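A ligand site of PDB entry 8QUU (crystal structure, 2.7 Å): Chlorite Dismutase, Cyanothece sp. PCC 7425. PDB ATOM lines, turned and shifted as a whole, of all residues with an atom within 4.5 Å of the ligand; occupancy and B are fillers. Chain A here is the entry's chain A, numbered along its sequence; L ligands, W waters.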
ATOM      1  N   ASN A  64      31.996  13.793  -7.247  1.00  0.00           N
ATOM      2  CA  ASN A  64      33.118  14.549  -7.767  1.00  0.00           C
ATOM      3  C   ASN A  64      32.758  16.009  -8.058  1.00  0.00           C
ATOM      4  O   ASN A  64      31.605  16.390  -8.265  1.00  0.00           O
ATOM      5  CB  ASN A  64      33.603  13.869  -9.056  1.00  0.00           C
ATOM      6  CG  ASN A  64      32.509  13.791 -10.111  1.00  0.00           C
ATOM      7  OD1 ASN A  64      31.586  12.965  -9.997  1.00  0.00           O
ATOM      8  ND2 ASN A  64      32.597  14.641 -11.123  1.00  0.00           N
ATOM      9  N   ILE A  65      33.806  16.822  -8.128  1.00  0.00           N
ATOM     10  CA  ILE A  65      33.694  18.249  -8.392  1.00  0.00           C
ATOM     11  C   ILE A  65      33.080  18.446  -9.772  1.00  0.00           C
ATOM     12  O   ILE A  65      33.475  17.752 -10.706  1.00  0.00           O
ATOM     13  CB  ILE A  65      35.090  18.881  -8.247  1.00  0.00           C
ATOM     14  CG1 ILE A  65      35.459  19.031  -6.779  1.00  0.00           C
ATOM     15  CG2 ILE A  65      35.200  20.199  -9.001  1.00  0.00           C
ATOM     16  CD1 ILE A  65      34.631  20.051  -6.041  1.00  0.00           C
ATOM     17  N   ARG A  66      32.144  19.399  -9.903  1.00  0.00           N
ATOM     18  CA  ARG A  66      31.490  19.677 -11.176  1.00  0.00           C
ATOM     19  C   ARG A  66      31.910  21.031 -11.797  1.00  0.00           C
ATOM     20  O   ARG A  66      31.805  21.167 -13.026  1.00  0.00           O
ATOM     21  CB  ARG A  66      29.966  19.621 -11.022  1.00  0.00           C
ATOM     22  CG  ARG A  66      29.437  18.408 -10.255  1.00  0.00           C
ATOM     23  CD  ARG A  66      29.807  17.061 -10.868  1.00  0.00           C
ATOM     24  NE  ARG A  66      29.162  15.910 -10.241  1.00  0.00           N
ATOM     25  CZ  ARG A  66      27.922  15.472 -10.489  1.00  0.00           C
ATOM     26  NH1 ARG A  66      27.193  15.998 -11.460  1.00  0.00           N
ATOM     27  NH2 ARG A  66      27.441  14.451  -9.783  1.00  0.00           N
ATOM     28  N   TYR A  67      32.350  22.036 -11.001  1.00  0.00           N
ATOM     29  CA  TYR A  67      32.580  23.393 -11.533  1.00  0.00           C
ATOM     30  C   TYR A  67      33.936  23.982 -11.111  1.00  0.00           C
ATOM     31  O   TYR A  67      34.601  24.666 -11.920  1.00  0.00           O
ATOM     32  CB  TYR A  67      31.466  24.376 -11.157  1.00  0.00           C
ATOM     33  CG  TYR A  67      30.115  24.021 -11.739  1.00  0.00           C
ATOM     34  CD1 TYR A  67      29.839  24.220 -13.083  1.00  0.00           C
ATOM     35  CD2 TYR A  67      29.140  23.408 -10.952  1.00  0.00           C
ATOM     36  CE1 TYR A  67      28.612  23.853 -13.621  1.00  0.00           C
ATOM     37  CE2 TYR A  67      27.918  23.017 -11.476  1.00  0.00           C
ATOM     38  CZ  TYR A  67      27.654  23.234 -12.820  1.00  0.00           C
ATOM     39  OH  TYR A  67      26.436  22.840 -13.320  1.00  0.00           O
ATOM     40  N   ALA A  68      34.346  23.768  -9.858  1.00  0.00           N
ATOM     41  CA  ALA A  68      35.574  24.348  -9.334  1.00  0.00           C
ATOM     42  C   ALA A  68      36.818  23.998 -10.162  1.00  0.00           C
ATOM     43  O   ALA A  68      37.052  22.842 -10.507  1.00  0.00           O
ATOM     44  CB  ALA A  68      35.745  23.872  -7.913  1.00  0.00           C
ATOM     45  N   LEU A  76      40.043  26.909  -1.418  1.00  0.00           N
ATOM     46  CA  LEU A  76      39.118  26.279  -0.499  1.00  0.00           C
ATOM     47  C   LEU A  76      39.871  25.411   0.508  1.00  0.00           C
ATOM     48  O   LEU A  76      39.562  25.461   1.683  1.00  0.00           O
ATOM     49  CB  LEU A  76      38.081  25.475  -1.301  1.00  0.00           C
ATOM     50  CG  LEU A  76      37.149  26.328  -2.163  1.00  0.00           C
ATOM     51  CD1 LEU A  76      36.498  25.517  -3.257  1.00  0.00           C
ATOM     52  CD2 LEU A  76      36.086  27.007  -1.318  1.00  0.00           C
ATOM     53  N   ILE A  94      19.810  22.832   3.641  1.00  0.00           N
ATOM     54  CA  ILE A  94      19.082  23.613   2.658  1.00  0.00           C
ATOM     55  C   ILE A  94      18.966  22.844   1.361  1.00  0.00           C
ATOM     56  O   ILE A  94      19.885  22.871   0.541  1.00  0.00           O
ATOM     57  CB  ILE A  94      19.684  25.013   2.399  1.00  0.00           C
ATOM     58  CG1 ILE A  94      19.965  25.761   3.709  1.00  0.00           C
ATOM     59  CG2 ILE A  94      18.782  25.809   1.475  1.00  0.00           C
ATOM     60  CD1 ILE A  94      20.684  27.065   3.507  1.00  0.00           C
ATOM     61  N   ILE A  96      17.720  22.340  -2.414  1.00  0.00           N
ATOM     62  CA  ILE A  96      17.590  23.234  -3.540  1.00  0.00           C
ATOM     63  C   ILE A  96      17.214  22.422  -4.775  1.00  0.00           C
ATOM     64  O   ILE A  96      17.824  21.389  -5.037  1.00  0.00           O
ATOM     65  CB  ILE A  96      18.911  23.986  -3.785  1.00  0.00           C
ATOM     66  CG1 ILE A  96      19.140  25.055  -2.727  1.00  0.00           C
ATOM     67  CG2 ILE A  96      18.956  24.572  -5.187  1.00  0.00           C
ATOM     68  CD1 ILE A  96      20.578  25.385  -2.523  1.00  0.00           C
ATOM     69  N   LYS A  98      16.912  23.299  -8.966  1.00  0.00           N
ATOM     70  CA  LYS A  98      17.098  24.233 -10.064  1.00  0.00           C
ATOM     71  C   LYS A  98      16.154  23.884 -11.220  1.00  0.00           C
ATOM     72  O   LYS A  98      15.591  22.794 -11.257  1.00  0.00           O
ATOM     73  CB  LYS A  98      18.563  24.198 -10.472  1.00  0.00           C
ATOM     74  CG  LYS A  98      19.531  24.732  -9.441  1.00  0.00           C
ATOM     75  CD  LYS A  98      20.854  25.154 -10.032  1.00  0.00           C
ATOM     76  CE  LYS A  98      21.831  25.683  -8.998  1.00  0.00           C
ATOM     77  NZ  LYS A  98      23.210  25.847  -9.532  1.00  0.00           N
ATOM     78  N   TRP A 102      17.929  25.439 -16.458  1.00  0.00           N
ATOM     79  CA  TRP A 102      19.295  25.301 -15.963  1.00  0.00           C
ATOM     80  C   TRP A 102      19.875  23.983 -16.445  1.00  0.00           C
ATOM     81  O   TRP A 102      20.957  23.970 -17.026  1.00  0.00           O
ATOM     82  CB  TRP A 102      19.371  25.386 -14.443  1.00  0.00           C
ATOM     83  CG  TRP A 102      20.712  25.028 -13.860  1.00  0.00           C
ATOM     84  CD1 TRP A 102      21.088  23.819 -13.331  1.00  0.00           C
ATOM     85  CD2 TRP A 102      21.863  25.890 -13.712  1.00  0.00           C
ATOM     86  NE1 TRP A 102      22.379  23.868 -12.898  1.00  0.00           N
ATOM     87  CE2 TRP A 102      22.875  25.118 -13.103  1.00  0.00           C
ATOM     88  CE3 TRP A 102      22.127  27.223 -14.027  1.00  0.00           C
ATOM     89  CZ2 TRP A 102      24.122  25.654 -12.794  1.00  0.00           C
ATOM     90  CZ3 TRP A 102      23.360  27.752 -13.726  1.00  0.00           C
ATOM     91  CH2 TRP A 102      24.353  26.965 -13.119  1.00  0.00           C
ATOM     92  N   PHE A 114      27.581  30.329 -12.773  1.00  0.00           N
ATOM     93  CA  PHE A 114      27.934  29.923 -11.424  1.00  0.00           C
ATOM     94  C   PHE A 114      29.077  30.793 -10.869  1.00  0.00           C
ATOM     95  O   PHE A 114      29.000  31.237  -9.716  1.00  0.00           O
ATOM     96  CB  PHE A 114      28.265  28.427 -11.419  1.00  0.00           C
ATOM     97  CG  PHE A 114      28.770  27.905 -10.096  1.00  0.00           C
ATOM     98  CD1 PHE A 114      27.875  27.516  -9.104  1.00  0.00           C
ATOM     99  CD2 PHE A 114      30.122  27.816  -9.843  1.00  0.00           C
ATOM    100  CE1 PHE A 114      28.326  27.059  -7.881  1.00  0.00           C
ATOM    101  CE2 PHE A 114      30.574  27.363  -8.611  1.00  0.00           C
ATOM    102  CZ  PHE A 114      29.682  26.994  -7.630  1.00  0.00           C
ATOM    103  N   HIS A 120      30.012  32.499  -7.031  1.00  0.00           N
ATOM    104  CA  HIS A 120      29.595  31.588  -5.956  1.00  0.00           C
ATOM    105  C   HIS A 120      30.766  31.268  -5.009  1.00  0.00           C
ATOM    106  O   HIS A 120      30.609  31.342  -3.809  1.00  0.00           O
ATOM    107  CB  HIS A 120      28.956  30.318  -6.517  1.00  0.00           C
ATOM    108  CG  HIS A 120      28.383  29.387  -5.490  1.00  0.00           C
ATOM    109  ND1 HIS A 120      27.045  29.113  -5.445  1.00  0.00           N
ATOM    110  CD2 HIS A 120      28.955  28.653  -4.488  1.00  0.00           C
ATOM    111  CE1 HIS A 120      26.817  28.263  -4.448  1.00  0.00           C
ATOM    112  NE2 HIS A 120      27.946  27.979  -3.848  1.00  0.00           N
ATOM    113  N   THR A 121      31.924  30.902  -5.551  1.00  0.00           N
ATOM    114  CA  THR A 121      33.033  30.439  -4.739  1.00  0.00           C
ATOM    115  C   THR A 121      33.735  31.612  -4.049  1.00  0.00           C
ATOM    116  O   THR A 121      34.023  31.561  -2.865  1.00  0.00           O
ATOM    117  CB  THR A 121      34.013  29.607  -5.575  1.00  0.00           C
ATOM    118  OG1 THR A 121      33.308  28.591  -6.305  1.00  0.00           O
ATOM    119  CG2 THR A 121      35.048  28.931  -4.701  1.00  0.00           C
ATOM    120  N   GLY A 124      31.437  32.732  -1.263  1.00  0.00           N
ATOM    121  CA  GLY A 124      31.392  31.735  -0.208  1.00  0.00           C
ATOM    122  C   GLY A 124      32.663  31.690   0.629  1.00  0.00           C
ATOM    123  O   GLY A 124      32.582  31.478   1.842  1.00  0.00           O
ATOM    124  N   LEU A 125      33.815  31.903  -0.021  1.00  0.00           N
ATOM    125  CA  LEU A 125      35.123  31.954   0.626  1.00  0.00           C
ATOM    126  C   LEU A 125      35.217  33.058   1.686  1.00  0.00           C
ATOM    127  O   LEU A 125      36.008  32.975   2.617  1.00  0.00           O
ATOM    128  CB  LEU A 125      36.196  32.149  -0.442  1.00  0.00           C
ATOM    129  CG  LEU A 125      37.009  30.902  -0.782  1.00  0.00           C
ATOM    130  CD1 LEU A 125      37.987  31.191  -1.907  1.00  0.00           C
ATOM    131  CD2 LEU A 125      37.765  30.393   0.439  1.00  0.00           C
ATOM    132  N   LEU A 128      34.429  31.604   5.206  1.00  0.00           N
ATOM    133  CA  LEU A 128      35.283  30.542   5.754  1.00  0.00           C
ATOM    134  C   LEU A 128      36.396  31.197   6.564  1.00  0.00           C
ATOM    135  O   LEU A 128      36.781  32.302   6.182  1.00  0.00           O
ATOM    136  CB  LEU A 128      35.838  29.745   4.570  1.00  0.00           C
ATOM    137  CG  LEU A 128      35.065  28.472   4.234  1.00  0.00           C
ATOM    138  CD1 LEU A 128      33.586  28.739   4.143  1.00  0.00           C
ATOM    139  CD2 LEU A 128      35.560  27.860   2.931  1.00  0.00           C
ATOM    140  N   VAL A 131      32.208  28.960   8.670  1.00  0.00           N
ATOM    141  CA  VAL A 131      31.219  27.991   8.171  1.00  0.00           C
ATOM    142  C   VAL A 131      31.849  26.738   7.559  1.00  0.00           C
ATOM    143  O   VAL A 131      32.588  26.793   6.576  1.00  0.00           O
ATOM    144  CB  VAL A 131      30.288  28.623   7.120  1.00  0.00           C
ATOM    145  CG1 VAL A 131      29.252  27.609   6.648  1.00  0.00           C
ATOM    146  CG2 VAL A 131      29.622  29.904   7.616  1.00  0.00           C
ATOM    147  N   ARG A 133      30.764  23.065   5.535  1.00  0.00           N
ATOM    148  CA  ARG A 133      29.738  22.752   4.547  1.00  0.00           C
ATOM    149  C   ARG A 133      29.902  21.318   4.015  1.00  0.00           C
ATOM    150  O   ARG A 133      30.981  20.767   4.023  1.00  0.00           O
ATOM    151  CB  ARG A 133      29.775  23.755   3.398  1.00  0.00           C
ATOM    152  CG  ARG A 133      30.944  23.583   2.443  1.00  0.00           C
ATOM    153  CD  ARG A 133      31.104  24.744   1.464  1.00  0.00           C
ATOM    154  NE  ARG A 133      32.002  24.381   0.377  1.00  0.00           N
ATOM    155  CZ  ARG A 133      33.329  24.295   0.460  1.00  0.00           C
ATOM    156  NH1 ARG A 133      33.968  24.687   1.554  1.00  0.00           N
ATOM    157  NH2 ARG A 133      34.041  23.818  -0.542  1.00  0.00           N
ATOM    158  N   LEU A 135      28.187  19.047   0.518  1.00  0.00           N
ATOM    159  CA  LEU A 135      27.302  19.116  -0.629  1.00  0.00           C
ATOM    160  C   LEU A 135      26.960  17.714  -1.125  1.00  0.00           C
ATOM    161  O   LEU A 135      27.829  16.875  -1.383  1.00  0.00           O
ATOM    162  CB  LEU A 135      27.962  19.918  -1.740  1.00  0.00           C
ATOM    163  CG  LEU A 135      27.208  19.907  -3.067  1.00  0.00           C
ATOM    164  CD1 LEU A 135      25.859  20.545  -2.946  1.00  0.00           C
ATOM    165  CD2 LEU A 135      28.012  20.596  -4.159  1.00  0.00           C
ATOM    166  N   HIS A 137      24.260  15.560  -3.900  1.00  0.00           N
ATOM    167  CA  HIS A 137      23.533  15.584  -5.157  1.00  0.00           C
ATOM    168  C   HIS A 137      22.389  14.584  -5.060  1.00  0.00           C
ATOM    169  O   HIS A 137      22.589  13.526  -4.431  1.00  0.00           O
ATOM    170  CB  HIS A 137      24.487  15.158  -6.280  1.00  0.00           C
ATOM    171  CG  HIS A 137      25.662  16.052  -6.423  1.00  0.00           C
ATOM    172  ND1 HIS A 137      25.743  17.016  -7.417  1.00  0.00           N
ATOM    173  CD2 HIS A 137      26.787  16.164  -5.673  1.00  0.00           C
ATOM    174  CE1 HIS A 137      26.906  17.657  -7.274  1.00  0.00           C
ATOM    175  NE2 HIS A 137      27.543  17.164  -6.202  1.00  0.00           N
ATOM    176  N   PHE A 147      19.529  19.053  -4.852  1.00  0.00           N
ATOM    177  CA  PHE A 147      20.686  19.112  -3.984  1.00  0.00           C
ATOM    178  C   PHE A 147      20.291  19.246  -2.519  1.00  0.00           C
ATOM    179  O   PHE A 147      19.299  19.870  -2.195  1.00  0.00           O
ATOM    180  CB  PHE A 147      21.607  20.327  -4.241  1.00  0.00           C
ATOM    181  CG  PHE A 147      22.038  20.547  -5.672  1.00  0.00           C
ATOM    182  CD1 PHE A 147      23.032  19.775  -6.246  1.00  0.00           C
ATOM    183  CD2 PHE A 147      21.447  21.534  -6.433  1.00  0.00           C
ATOM    184  CE1 PHE A 147      23.421  19.996  -7.561  1.00  0.00           C
ATOM    185  CE2 PHE A 147      21.831  21.743  -7.753  1.00  0.00           C
ATOM    186  CZ  PHE A 147      22.805  20.962  -8.321  1.00  0.00           C
ATOM    187  N   THR A 149      22.244  20.757   0.795  1.00  0.00           N
ATOM    188  CA  THR A 149      23.414  21.478   1.224  1.00  0.00           C
ATOM    189  C   THR A 149      23.366  21.513   2.734  1.00  0.00           C
ATOM    190  O   THR A 149      22.301  21.515   3.320  1.00  0.00           O
ATOM    191  CB  THR A 149      23.499  22.861   0.573  1.00  0.00           C
ATOM    192  OG1 THR A 149      22.484  23.741   1.067  1.00  0.00           O
ATOM    193  CG2 THR A 149      23.413  22.766  -0.930  1.00  0.00           C
ATOM    194  N   PHE A 151      25.432  23.073   6.277  1.00  0.00           N
ATOM    195  CA  PHE A 151      26.285  24.112   6.815  1.00  0.00           C
ATOM    196  C   PHE A 151      26.258  24.025   8.332  1.00  0.00           C
ATOM    197  O   PHE A 151      25.172  23.904   8.894  1.00  0.00           O
ATOM    198  CB  PHE A 151      25.805  25.505   6.419  1.00  0.00           C
ATOM    199  CG  PHE A 151      25.632  25.613   4.936  1.00  0.00           C
ATOM    200  CD1 PHE A 151      26.729  25.800   4.121  1.00  0.00           C
ATOM    201  CD2 PHE A 151      24.394  25.373   4.364  1.00  0.00           C
ATOM    202  CE1 PHE A 151      26.574  25.848   2.749  1.00  0.00           C
ATOM    203  CE2 PHE A 151      24.257  25.348   2.985  1.00  0.00           C
ATOM    204  CZ  PHE A 151      25.337  25.612   2.187  1.00  0.00           C
ATOM    205  N   PHE A 161      26.258  34.018   8.502  1.00  0.00           N
ATOM    206  CA  PHE A 161      25.632  33.004   7.664  1.00  0.00           C
ATOM    207  C   PHE A 161      24.377  33.573   7.009  1.00  0.00           C
ATOM    208  O   PHE A 161      24.142  33.327   5.812  1.00  0.00           O
ATOM    209  CB  PHE A 161      25.326  31.705   8.431  1.00  0.00           C
ATOM    210  CG  PHE A 161      24.787  30.630   7.530  1.00  0.00           C
ATOM    211  CD1 PHE A 161      25.612  29.985   6.624  1.00  0.00           C
ATOM    212  CD2 PHE A 161      23.417  30.345   7.492  1.00  0.00           C
ATOM    213  CE1 PHE A 161      25.101  29.055   5.723  1.00  0.00           C
ATOM    214  CE2 PHE A 161      22.912  29.396   6.612  1.00  0.00           C
ATOM    215  CZ  PHE A 161      23.756  28.770   5.717  1.00  0.00           C
ATOM    216  N   LEU A 164      25.330  35.735   4.200  1.00  0.00           N
ATOM    217  CA  LEU A 164      25.677  34.905   3.046  1.00  0.00           C
ATOM    218  C   LEU A 164      24.420  34.430   2.284  1.00  0.00           C
ATOM    219  O   LEU A 164      24.379  34.533   1.058  1.00  0.00           O
ATOM    220  CB  LEU A 164      26.575  33.756   3.501  1.00  0.00           C
ATOM    221  CG  LEU A 164      26.783  32.617   2.489  1.00  0.00           C
ATOM    222  CD1 LEU A 164      27.624  33.067   1.296  1.00  0.00           C
ATOM    223  CD2 LEU A 164      27.400  31.403   3.178  1.00  0.00           C
ATOM    224  N   LEU A 165      23.365  33.960   2.976  1.00  0.00           N
ATOM    225  CA  LEU A 165      22.178  33.473   2.285  1.00  0.00           C
ATOM    226  C   LEU A 165      21.590  34.543   1.387  1.00  0.00           C
ATOM    227  O   LEU A 165      21.153  34.240   0.279  1.00  0.00           O
ATOM    228  CB  LEU A 165      21.106  33.070   3.283  1.00  0.00           C
ATOM    229  CG  LEU A 165      21.322  31.766   4.056  1.00  0.00           C
ATOM    230  CD1 LEU A 165      20.227  31.606   5.107  1.00  0.00           C
ATOM    231  CD2 LEU A 165      21.347  30.542   3.135  1.00  0.00           C
ATOM    232  N   MET A 168      23.665  35.160  -1.847  1.00  0.00           N
ATOM    233  CA  MET A 168      23.564  34.111  -2.845  1.00  0.00           C
ATOM    234  C   MET A 168      22.244  34.268  -3.604  1.00  0.00           C
ATOM    235  O   MET A 168      22.204  34.135  -4.827  1.00  0.00           O
ATOM    236  CB  MET A 168      23.623  32.731  -2.192  1.00  0.00           C
ATOM    237  CG  MET A 168      24.977  32.333  -1.613  1.00  0.00           C
ATOM    238  SD  MET A 168      26.201  32.029  -2.886  1.00  0.00           S
ATOM    239  CE  MET A 168      27.410  31.056  -1.987  1.00  0.00           C
ATOM    240  N   GLU A 173      22.760  33.112 -10.512  1.00  0.00           N
ATOM    241  CA  GLU A 173      22.554  31.699 -10.281  1.00  0.00           C
ATOM    242  C   GLU A 173      21.149  31.446  -9.720  1.00  0.00           C
ATOM    243  O   GLU A 173      20.486  30.495 -10.145  1.00  0.00           O
ATOM    244  CB  GLU A 173      23.599  31.141  -9.312  1.00  0.00           C
ATOM    245  CG  GLU A 173      23.596  29.614  -9.202  1.00  0.00           C
ATOM    246  CD  GLU A 173      24.553  29.044  -8.153  1.00  0.00           C
ATOM    247  OE1 GLU A 173      25.212  29.847  -7.466  1.00  0.00           O
ATOM    248  OE2 GLU A 173      24.628  27.778  -8.019  1.00  0.00           O
ATOM    249  N   TRP A 174      20.708  32.272  -8.764  1.00  0.00           N
ATOM    250  CA  TRP A 174      19.512  31.942  -7.991  1.00  0.00           C
ATOM    251  C   TRP A 174      18.225  32.209  -8.755  1.00  0.00           C
ATOM    252  O   TRP A 174      17.165  31.860  -8.264  1.00  0.00           O
ATOM    253  CB  TRP A 174      19.500  32.630  -6.620  1.00  0.00           C
ATOM    254  CG  TRP A 174      19.526  31.626  -5.486  1.00  0.00           C
ATOM    255  CD1 TRP A 174      18.460  31.250  -4.719  1.00  0.00           C
ATOM    256  CD2 TRP A 174      20.661  30.881  -5.002  1.00  0.00           C
ATOM    257  NE1 TRP A 174      18.854  30.326  -3.798  1.00  0.00           N
ATOM    258  CE2 TRP A 174      20.195  30.084  -3.939  1.00  0.00           C
ATOM    259  CE3 TRP A 174      22.018  30.815  -5.342  1.00  0.00           C
ATOM    260  CZ2 TRP A 174      21.042  29.221  -3.226  1.00  0.00           C
ATOM    261  CZ3 TRP A 174      22.860  29.987  -4.624  1.00  0.00           C
ATOM    262  CH2 TRP A 174      22.376  29.185  -3.593  1.00  0.00           C
ATOM    263  N   GLU A 180      13.251  25.875  -2.551  1.00  0.00           N
ATOM    264  CA  GLU A 180      14.244  26.077  -1.511  1.00  0.00           C
ATOM    265  C   GLU A 180      13.566  26.032  -0.149  1.00  0.00           C
ATOM    266  O   GLU A 180      12.464  26.559   0.006  1.00  0.00           O
ATOM    267  CB  GLU A 180      14.982  27.380  -1.737  1.00  0.00           C
ATOM    268  CG  GLU A 180      16.132  27.604  -0.787  1.00  0.00           C
ATOM    269  CD  GLU A 180      17.002  28.803  -1.111  1.00  0.00           C
ATOM    270  OE1 GLU A 180      16.682  29.559  -2.105  1.00  0.00           O
ATOM    271  OE2 GLU A 180      18.006  28.993  -0.362  1.00  0.00           O
HETATM  272  C1  LIG L   1      28.288  24.247  -5.161  1.00  0.00           C
HETATM  273  C2  LIG L   1      31.387  26.594  -2.367  1.00  0.00           C
HETATM  274  C3  LIG L   1      27.818  28.250   0.374  1.00  0.00           C
HETATM  275  C4  LIG L   1      24.678  26.187  -2.652  1.00  0.00           C
HETATM  276  C5  LIG L   1      29.435  24.798  -4.627  1.00  0.00           C
HETATM  277  C6  LIG L   1      30.717  24.651  -5.227  1.00  0.00           C
HETATM  278  C7  LIG L   1      31.582  25.313  -4.418  1.00  0.00           C
HETATM  279  C8  LIG L   1      30.839  25.860  -3.361  1.00  0.00           C
HETATM  280  C9  LIG L   1      33.075  25.471  -4.625  1.00  0.00           C
HETATM  281  C10 LIG L   1      31.075  23.927  -6.495  1.00  0.00           C
HETATM  282  C11 LIG L   1      31.155  22.421  -6.289  1.00  0.00           C
HETATM  283  C12 LIG L   1      31.613  21.673  -7.539  1.00  0.00           C
HETATM  284  O1  LIG L   1      31.211  20.503  -7.645  1.00  0.00           O
HETATM  285  O2  LIG L   1      32.366  22.156  -8.459  1.00  0.00           O
HETATM  286  C13 LIG L   1      30.668  27.190  -1.383  1.00  0.00           C
HETATM  287  C14 LIG L   1      31.317  27.868  -0.354  1.00  0.00           C
HETATM  288  C15 LIG L   1      30.351  28.349   0.445  1.00  0.00           C
HETATM  289  C16 LIG L   1      29.068  27.933  -0.131  1.00  0.00           C
HETATM  290  C17 LIG L   1      32.797  28.041  -0.079  1.00  0.00           C
HETATM  291  C18 LIG L   1      30.688  29.007   1.697  1.00  0.00           C
HETATM  292  C19 LIG L   1      29.833  28.928   2.701  1.00  0.00           C
HETATM  293  C20 LIG L   1      26.632  27.875  -0.242  1.00  0.00           C
HETATM  294  C21 LIG L   1      25.326  28.138   0.217  1.00  0.00           C
HETATM  295  C22 LIG L   1      24.454  27.527  -0.631  1.00  0.00           C
HETATM  296  C23 LIG L   1      25.232  26.907  -1.628  1.00  0.00           C
HETATM  297  C24 LIG L   1      24.925  28.910   1.439  1.00  0.00           C
HETATM  298  C25 LIG L   1      22.984  27.495  -0.629  1.00  0.00           C
HETATM  299  C26 LIG L   1      22.219  28.136   0.230  1.00  0.00           C
HETATM  300  C27 LIG L   1      25.442  25.464  -3.558  1.00  0.00           C
HETATM  301  C28 LIG L   1      24.841  24.563  -4.549  1.00  0.00           C
HETATM  302  C29 LIG L   1      25.850  24.039  -5.247  1.00  0.00           C
HETATM  303  C30 LIG L   1      27.054  24.581  -4.632  1.00  0.00           C
HETATM  304  C31 LIG L   1      23.357  24.293  -4.805  1.00  0.00           C
HETATM  305  C32 LIG L   1      25.725  23.075  -6.369  1.00  0.00           C
HETATM  306  C33 LIG L   1      25.538  23.793  -7.680  1.00  0.00           C
HETATM  307  C34 LIG L   1      25.455  22.809  -8.828  1.00  0.00           C
HETATM  308  O3  LIG L   1      26.146  21.724  -8.839  1.00  0.00           O
HETATM  309  O4  LIG L   1      24.680  23.117  -9.757  1.00  0.00           O
HETATM  310  N1  LIG L   1      29.520  25.551  -3.469  1.00  0.00           N
HETATM  311  N2  LIG L   1      29.369  27.239  -1.208  1.00  0.00           N
HETATM  312  N3  LIG L   1      26.542  27.156  -1.350  1.00  0.00           N
HETATM  313  N4  LIG L   1      26.769  25.432  -3.618  1.00  0.00           N
HETATM  314 FE1  LIG L   1      28.004  26.368  -2.501  1.00  0.00          FE
HETATM  315  O   HOH W   1      28.460  23.874  -0.870  1.00  0.00           O
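NE2 of His 120 binds FE1 of the ligand, 2.1 Å away.
The backbone NH (N) of Tyr 67 lies within hydrogen-bond range of an oxygen (O2) of the ligand (2.5 Å).
The backbone NH (N) of Arg 66 sits at hydrogen-bond distance from an oxygen (O1) of the ligand (2.7 Å).
An oxygen (O2) of the ligand is in hydrogen-bond range of the backbone NH of Ala 68, 2.9 Å away.
NZ of Lys 98 is in salt-bridge range of O4 of the ligand (3.1 Å).
O of Phe 114 lies within hydrogen-bond range of N of His 120.
ND1 of His 120 lies within hydrogen-bond range of OE1 of Glu 173 (2.8 Å).
NE of Arg 66 lies within hydrogen-bond range of O of Asn 64, 3.2 Å away.
The side-chain amino group (NZ) of Lys 98 lies within salt-bridge range of the side-chain carboxylate (OE2) of Glu 173.
The backbone carbonyl oxygen (O) of Ile 96 sits at hydrogen-bond distance from the backbone NH (N) of Phe 147, at 2.9 Å.
The indole nitrogen of Trp 174 sits at hydrogen-bond distance from the side-chain carboxylate of Glu 180 (2.9 Å).
The backbone carbonyl oxygen of Ile 94 sits at hydrogen-bond distance from the side-chain hydroxyl of Thr 149 (2.8 Å).
Merely in contact with the ligand: Gly 124 (3.1 Å), Phe 147 (3.2 Å), Phe 151 (3.2 Å), Ile 65 (3.4 Å), Trp 174 (3.5 Å), Leu 164 (3.5 Å), Phe 114 (3.5 Å), Thr 121 (3.6 Å), Arg 133 (3.6 Å), Leu 76 (3.7 Å), Met 168 (3.7 Å), Ile 96 (3.7 Å), Ile 94 (3.8 Å), Leu 135 (3.8 Å), Leu 128 (3.8 Å), Leu 165 (3.9 Å), Trp 102 (3.97 Å) and Leu 125 (3.99 Å).
Hydrophobic or aromatic side chains that line the ligand: Ile 65, Tyr 67, Ala 68, Leu 76, Ile 94, Ile 96, Trp 102, Phe 114, His 120, Leu 128, Leu 135, Phe 147, Phe 151, Leu 164, Leu 165, Met 168 and Trp 174.
Within 4 Å of the ligand: Ile 65, Arg 66, Tyr 67, Ala 68, Leu 76, Ile 94, Ile 96, Lys 98, Trp 102, Phe 114, His 120, Thr 121, Gly 124, Leu 125, Leu 128, Arg 133, Leu 135, Phe 147, Phe 151, Leu 164, Leu 165, Met 168 and Trp 174.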
